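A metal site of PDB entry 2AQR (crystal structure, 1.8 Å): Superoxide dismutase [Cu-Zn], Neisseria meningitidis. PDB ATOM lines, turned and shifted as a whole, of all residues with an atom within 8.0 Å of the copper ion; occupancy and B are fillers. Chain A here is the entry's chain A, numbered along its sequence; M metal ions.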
ATOM      1  N   GLY A  55      18.370  17.111  19.076  1.00  0.00           N
ATOM      2  CA  GLY A  55      19.113  18.367  19.129  1.00  0.00           C
ATOM      3  C   GLY A  55      19.988  18.399  17.897  1.00  0.00           C
ATOM      4  O   GLY A  55      20.627  17.399  17.550  1.00  0.00           O
ATOM      5  N   PHE A  56      20.066  19.561  17.261  1.00  0.00           N
ATOM      6  CA  PHE A  56      20.822  19.710  16.024  1.00  0.00           C
ATOM      7  C   PHE A  56      21.582  21.037  16.091  1.00  0.00           C
ATOM      8  O   PHE A  56      20.961  22.100  16.070  1.00  0.00           O
ATOM      9  CB  PHE A  56      19.784  19.692  14.888  1.00  0.00           C
ATOM     10  CG  PHE A  56      20.347  19.551  13.505  1.00  0.00           C
ATOM     11  CD1 PHE A  56      21.420  18.705  13.243  1.00  0.00           C
ATOM     12  CD2 PHE A  56      19.705  20.182  12.438  1.00  0.00           C
ATOM     13  CE1 PHE A  56      21.848  18.491  11.929  1.00  0.00           C
ATOM     14  CE2 PHE A  56      20.119  19.967  11.127  1.00  0.00           C
ATOM     15  CZ  PHE A  56      21.192  19.121  10.866  1.00  0.00           C
ATOM     16  N   HIS A  57      22.905  20.975  16.193  1.00  0.00           N
ATOM     17  CA  HIS A  57      23.681  22.213  16.294  1.00  0.00           C
ATOM     18  C   HIS A  57      25.034  22.170  15.606  1.00  0.00           C
ATOM     19  O   HIS A  57      25.590  21.104  15.334  1.00  0.00           O
ATOM     20  CB  HIS A  57      23.965  22.576  17.753  1.00  0.00           C
ATOM     21  CG  HIS A  57      22.968  22.045  18.733  1.00  0.00           C
ATOM     22  ND1 HIS A  57      23.223  20.965  19.542  1.00  0.00           N
ATOM     23  CD2 HIS A  57      21.717  22.468  19.055  1.00  0.00           C
ATOM     24  CE1 HIS A  57      22.171  20.734  20.315  1.00  0.00           C
ATOM     25  NE2 HIS A  57      21.256  21.641  20.043  1.00  0.00           N
ATOM     26  N   ILE A  58      25.553  23.358  15.339  1.00  0.00           N
ATOM     27  CA  ILE A  58      26.880  23.503  14.763  1.00  0.00           C
ATOM     28  C   ILE A  58      27.798  23.622  15.974  1.00  0.00           C
ATOM     29  O   ILE A  58      27.561  24.462  16.849  1.00  0.00           O
ATOM     30  CB  ILE A  58      27.007  24.814  13.946  1.00  0.00           C
ATOM     31  CG1 ILE A  58      26.007  24.824  12.790  1.00  0.00           C
ATOM     32  CG2 ILE A  58      28.440  24.972  13.415  1.00  0.00           C
ATOM     33  CD1 ILE A  58      26.232  23.723  11.768  1.00  0.00           C
ATOM     34  N   HIS A  59      28.816  22.773  16.051  1.00  0.00           N
ATOM     35  CA  HIS A  59      29.765  22.844  17.149  1.00  0.00           C
ATOM     36  C   HIS A  59      31.047  23.517  16.677  1.00  0.00           C
ATOM     37  O   HIS A  59      31.350  23.518  15.489  1.00  0.00           O
ATOM     38  CB  HIS A  59      30.049  21.451  17.738  1.00  0.00           C
ATOM     39  CG  HIS A  59      28.933  20.941  18.594  1.00  0.00           C
ATOM     40  ND1 HIS A  59      29.114  20.565  19.899  1.00  0.00           N
ATOM     41  CD2 HIS A  59      27.617  20.782  18.332  1.00  0.00           C
ATOM     42  CE1 HIS A  59      27.956  20.195  20.415  1.00  0.00           C
ATOM     43  NE2 HIS A  59      27.025  20.329  19.484  1.00  0.00           N
ATOM     44  N   ALA A  79      34.480  17.656  19.086  1.00  0.00           N
ATOM     45  CA  ALA A  79      33.808  18.750  18.392  1.00  0.00           C
ATOM     46  C   ALA A  79      33.711  20.026  19.232  1.00  0.00           C
ATOM     47  O   ALA A  79      33.436  21.105  18.698  1.00  0.00           O
ATOM     48  CB  ALA A  79      32.409  18.319  17.956  1.00  0.00           C
ATOM     49  N   GLY A  80      33.931  19.911  20.529  1.00  0.00           N
ATOM     50  CA  GLY A  80      33.835  21.073  21.400  1.00  0.00           C
ATOM     51  C   GLY A  80      32.389  21.412  21.693  1.00  0.00           C
ATOM     52  O   GLY A  80      31.486  20.585  21.482  1.00  0.00           O
ATOM     53  N   GLY A  81      32.136  22.625  22.167  1.00  0.00           N
ATOM     54  CA  GLY A  81      30.779  23.021  22.496  1.00  0.00           C
ATOM     55  C   GLY A  81      30.046  23.653  21.330  1.00  0.00           C
ATOM     56  O   GLY A  81      30.523  23.639  20.193  1.00  0.00           O
ATOM     57  N   HIS A  82      28.862  24.206  21.602  1.00  0.00           N
ATOM     58  CA  HIS A  82      28.093  24.840  20.550  1.00  0.00           C
ATOM     59  C   HIS A  82      28.854  26.041  20.000  1.00  0.00           C
ATOM     60  O   HIS A  82      29.429  26.828  20.768  1.00  0.00           O
ATOM     61  CB  HIS A  82      26.735  25.305  21.089  1.00  0.00           C
ATOM     62  CG  HIS A  82      25.835  24.195  21.526  1.00  0.00           C
ATOM     63  ND1 HIS A  82      24.499  24.383  21.788  1.00  0.00           N
ATOM     64  CD2 HIS A  82      26.081  22.882  21.758  1.00  0.00           C
ATOM     65  CE1 HIS A  82      23.960  23.231  22.149  1.00  0.00           C
ATOM     66  NE2 HIS A  82      24.898  22.308  22.134  1.00  0.00           N
ATOM     67  N   TRP A  83      28.871  26.185  18.687  1.00  0.00           N
ATOM     68  CA  TRP A  83      29.564  27.304  18.064  1.00  0.00           C
ATOM     69  C   TRP A  83      28.936  28.599  18.556  1.00  0.00           C
ATOM     70  O   TRP A  83      27.748  28.848  18.354  1.00  0.00           O
ATOM     71  CB  TRP A  83      29.486  27.196  16.535  1.00  0.00           C
ATOM     72  CG  TRP A  83      30.330  28.203  15.838  1.00  0.00           C
ATOM     73  CD1 TRP A  83      31.606  28.574  16.154  1.00  0.00           C
ATOM     74  CD2 TRP A  83      29.965  28.980  14.687  1.00  0.00           C
ATOM     75  NE1 TRP A  83      32.063  29.526  15.274  1.00  0.00           N
ATOM     76  CE2 TRP A  83      31.076  29.787  14.355  1.00  0.00           C
ATOM     77  CE3 TRP A  83      28.808  29.055  13.901  1.00  0.00           C
ATOM     78  CZ2 TRP A  83      31.062  30.679  13.275  1.00  0.00           C
ATOM     79  CZ3 TRP A  83      28.800  29.935  12.817  1.00  0.00           C
ATOM     80  CH2 TRP A  83      29.920  30.734  12.518  1.00  0.00           C
ATOM     81  N   HIS A  91      22.229  28.894  25.410  1.00  0.00           N
ATOM     82  CA  HIS A  91      21.590  28.084  24.381  1.00  0.00           C
ATOM     83  C   HIS A  91      20.174  28.620  24.159  1.00  0.00           C
ATOM     84  O   HIS A  91      19.484  28.938  25.124  1.00  0.00           O
ATOM     85  CB  HIS A  91      21.527  26.627  24.799  1.00  0.00           C
ATOM     86  CG  HIS A  91      20.943  25.725  23.756  1.00  0.00           C
ATOM     87  ND1 HIS A  91      21.592  25.459  22.569  1.00  0.00           N
ATOM     88  CD2 HIS A  91      19.752  25.098  23.683  1.00  0.00           C
ATOM     89  CE1 HIS A  91      20.820  24.712  21.800  1.00  0.00           C
ATOM     90  NE2 HIS A  91      19.695  24.482  22.456  1.00  0.00           N
ATOM     91  N   GLY A 102      25.311  28.675  16.623  1.00  0.00           N
ATOM     92  CA  GLY A 102      25.203  27.325  16.098  1.00  0.00           C
ATOM     93  C   GLY A 102      23.899  26.602  16.390  1.00  0.00           C
ATOM     94  O   GLY A 102      23.731  25.452  15.988  1.00  0.00           O
ATOM     95  N   ASP A 103      22.966  27.271  17.067  1.00  0.00           N
ATOM     96  CA  ASP A 103      21.691  26.641  17.420  1.00  0.00           C
ATOM     97  C   ASP A 103      20.734  26.527  16.226  1.00  0.00           C
ATOM     98  O   ASP A 103      20.203  27.527  15.742  1.00  0.00           O
ATOM     99  CB  ASP A 103      21.005  27.396  18.568  1.00  0.00           C
ATOM    100  CG  ASP A 103      21.806  27.345  19.861  1.00  0.00           C
ATOM    101  OD1 ASP A 103      22.685  26.461  19.988  1.00  0.00           O
ATOM    102  OD2 ASP A 103      21.565  28.186  20.750  1.00  0.00           O
ATOM    103  N   SER A 134      31.676  21.704  12.842  1.00  0.00           N
ATOM    104  CA  SER A 134      31.035  20.397  12.756  1.00  0.00           C
ATOM    105  C   SER A 134      29.538  20.528  13.012  1.00  0.00           C
ATOM    106  O   SER A 134      29.083  21.515  13.569  1.00  0.00           O
ATOM    107  CB  SER A 134      31.650  19.444  13.786  1.00  0.00           C
ATOM    108  OG  SER A 134      31.623  20.011  15.088  1.00  0.00           O
ATOM    109  N   ILE A 135      28.782  19.536  12.560  1.00  0.00           N
ATOM    110  CA  ILE A 135      27.351  19.545  12.785  1.00  0.00           C
ATOM    111  C   ILE A 135      27.065  18.312  13.639  1.00  0.00           C
ATOM    112  O   ILE A 135      27.556  17.222  13.365  1.00  0.00           O
ATOM    113  CB  ILE A 135      26.576  19.535  11.445  1.00  0.00           C
ATOM    114  CG1 ILE A 135      25.079  19.724  11.704  1.00  0.00           C
ATOM    115  CG2 ILE A 135      26.858  18.253  10.674  1.00  0.00           C
ATOM    116  CD1 ILE A 135      24.305  20.129  10.475  1.00  0.00           C
ATOM    117  N   MET A 136      26.298  18.525  14.699  1.00  0.00           N
ATOM    118  CA  MET A 136      26.018  17.456  15.639  1.00  0.00           C
ATOM    119  C   MET A 136      24.541  17.110  15.780  1.00  0.00           C
ATOM    120  O   MET A 136      23.688  17.978  15.728  1.00  0.00           O
ATOM    121  CB  MET A 136      26.543  17.879  17.017  1.00  0.00           C
ATOM    122  CG  MET A 136      26.662  16.777  18.038  1.00  0.00           C
ATOM    123  SD  MET A 136      28.092  15.736  17.739  1.00  0.00           S
ATOM    124  CE  MET A 136      29.419  16.890  18.117  1.00  0.00           C
ATOM    125  N   ILE A 137      24.274  15.817  15.942  1.00  0.00           N
ATOM    126  CA  ILE A 137      22.912  15.323  16.157  1.00  0.00           C
ATOM    127  C   ILE A 137      22.992  14.611  17.508  1.00  0.00           C
ATOM    128  O   ILE A 137      23.792  13.701  17.703  1.00  0.00           O
ATOM    129  CB  ILE A 137      22.493  14.324  15.065  1.00  0.00           C
ATOM    130  CG1 ILE A 137      22.447  15.024  13.702  1.00  0.00           C
ATOM    131  CG2 ILE A 137      21.118  13.741  15.400  1.00  0.00           C
ATOM    132  CD1 ILE A 137      22.089  14.120  12.541  1.00  0.00           C
ATOM    133  N   HIS A 138      22.157  15.038  18.452  1.00  0.00           N
ATOM    134  CA  HIS A 138      22.165  14.474  19.787  1.00  0.00           C
ATOM    135  C   HIS A 138      21.149  13.370  19.991  1.00  0.00           C
ATOM    136  O   HIS A 138      20.238  13.184  19.185  1.00  0.00           O
ATOM    137  CB  HIS A 138      21.914  15.581  20.823  1.00  0.00           C
ATOM    138  CG  HIS A 138      23.013  16.594  20.894  1.00  0.00           C
ATOM    139  ND1 HIS A 138      24.021  16.527  21.842  1.00  0.00           N
ATOM    140  CD2 HIS A 138      23.298  17.658  20.118  1.00  0.00           C
ATOM    141  CE1 HIS A 138      24.867  17.517  21.656  1.00  0.00           C
ATOM    142  NE2 HIS A 138      24.457  18.226  20.614  1.00  0.00           N
ATOM    143  N   ASP A 142      15.631  19.093  21.990  1.00  0.00           N
ATOM    144  CA  ASP A 142      16.105  20.464  22.141  1.00  0.00           C
ATOM    145  C   ASP A 142      14.928  21.383  22.485  1.00  0.00           C
ATOM    146  O   ASP A 142      14.080  21.642  21.629  1.00  0.00           O
ATOM    147  CB  ASP A 142      16.779  20.949  20.848  1.00  0.00           C
ATOM    148  CG  ASP A 142      17.642  22.186  21.062  1.00  0.00           C
ATOM    149  OD1 ASP A 142      17.474  22.872  22.094  1.00  0.00           O
ATOM    150  OD2 ASP A 142      18.478  22.488  20.184  1.00  0.00           O
ATOM    151  N   LEU A 151      22.003  23.082  27.517  1.00  0.00           N
ATOM    152  CA  LEU A 151      22.033  22.897  26.070  1.00  0.00           C
ATOM    153  C   LEU A 151      20.798  22.231  25.463  1.00  0.00           C
ATOM    154  O   LEU A 151      20.896  21.369  24.586  1.00  0.00           O
ATOM    155  CB  LEU A 151      23.299  22.118  25.705  1.00  0.00           C
ATOM    156  CG  LEU A 151      24.571  22.748  26.281  1.00  0.00           C
ATOM    157  CD1 LEU A 151      25.752  21.798  26.125  1.00  0.00           C
ATOM    158  CD2 LEU A 151      24.848  24.075  25.603  1.00  0.00           C
ATOM    159  N   GLY A 154      19.902  18.122  24.935  1.00  0.00           N
ATOM    160  CA  GLY A 154      20.380  17.235  23.883  1.00  0.00           C
ATOM    161  C   GLY A 154      21.133  16.039  24.431  1.00  0.00           C
ATOM    162  O   GLY A 154      21.060  14.938  23.884  1.00  0.00           O
ATOM    163  N   GLY A 155      21.853  16.253  25.526  1.00  0.00           N
ATOM    164  CA  GLY A 155      22.607  15.153  26.113  1.00  0.00           C
ATOM    165  C   GLY A 155      23.704  14.622  25.222  1.00  0.00           C
ATOM    166  O   GLY A 155      24.357  15.390  24.509  1.00  0.00           O
ATOM    167  N   PRO A 156      23.931  13.297  25.228  1.00  0.00           N
ATOM    168  CA  PRO A 156      24.962  12.614  24.419  1.00  0.00           C
ATOM    169  C   PRO A 156      24.933  12.940  22.933  1.00  0.00           C
ATOM    170  O   PRO A 156      23.907  13.303  22.364  1.00  0.00           O
ATOM    171  CB  PRO A 156      24.687  11.138  24.688  1.00  0.00           C
ATOM    172  CG  PRO A 156      24.124  11.145  26.066  1.00  0.00           C
ATOM    173  CD  PRO A 156      23.176  12.323  26.023  1.00  0.00           C
ATOM    174  N   ARG A 157      26.095  12.785  22.293  1.00  0.00           N
ATOM    175  CA  ARG A 157      26.251  13.046  20.873  1.00  0.00           C
ATOM    176  C   ARG A 157      26.090  11.739  20.107  1.00  0.00           C
ATOM    177  O   ARG A 157      26.896  10.818  20.231  1.00  0.00           O
ATOM    178  CB  ARG A 157      27.614  13.700  20.640  1.00  0.00           C
ATOM    179  CG  ARG A 157      27.723  14.975  21.459  1.00  0.00           C
ATOM    180  CD  ARG A 157      29.078  15.642  21.459  1.00  0.00           C
ATOM    181  NE  ARG A 157      29.070  16.760  22.388  1.00  0.00           N
ATOM    182  CZ  ARG A 157      29.944  17.761  22.401  1.00  0.00           C
ATOM    183  NH1 ARG A 157      30.932  17.777  21.506  1.00  0.00           N
ATOM    184  NH2 ARG A 157      29.832  18.739  23.288  1.00  0.00           N
ATOM    185  N   ALA A 159      25.296  11.458  16.412  1.00  0.00           N
ATOM    186  CA  ALA A 159      25.868  11.466  15.072  1.00  0.00           C
ATOM    187  C   ALA A 159      26.565  12.801  14.825  1.00  0.00           C
ATOM    188  O   ALA A 159      26.231  13.804  15.460  1.00  0.00           O
ATOM    189  CB  ALA A 159      24.778  11.234  14.040  1.00  0.00           C
HETATM  190 CU    CU M   1      25.064  19.992  19.786  1.00  0.00          CU
HETATM  191 ZN    ZN M   2      23.392  26.073  21.743  1.00  0.00          ZN
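O of Gly 80 is in hydrogen-bond range of ND1 of His 59 (2.9 Å).
A ring nitrogen (ND1) of His 57 sits close to a ring nitrogen (NE2) of His 82, at 3.4 Å.
A ring nitrogen (ND1) of His 138 lies within hydrogen-bond range of the backbone carbonyl oxygen (O) of Gly 155.
The backbone NH of His 59 lies within hydrogen-bond range of the backbone carbonyl oxygen of Ser 134 (2.8 Å).
A ring nitrogen (ND1) of His 138 lies within hydrogen-bond range of the backbone carbonyl oxygen (O) of Pro 156, 3.3 Å away.
A ring nitrogen (ND1) of His 59 lies close to the backbone carbonyl oxygen (O) of Gly 81, at 3.4 Å.
The backbone NH (N) of His 138 is in hydrogen-bond range of the backbone carbonyl oxygen (O) of Gly 55, at 3.0 Å.
OD2 of Asp 142 lies within hydrogen-bond range of NE2 of His 57.
NE2 of His 82 touches the copper ion, at 3.3 Å.
CB of Met 136 touches the copper ion, at 3.8 Å.
Of the 25 residues printed, 5 come within 4 Å of the copper ion.
The nearest printed residue that does not touch the copper ion is Phe 56 (5.2 Å).
The copper ion is bound by a ring nitrogen (NE2) of His 59, a ring nitrogen (NE2) of His 138 and a ring nitrogen (ND1) of His 57.
The copper ion has three donor atoms within binding distance.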
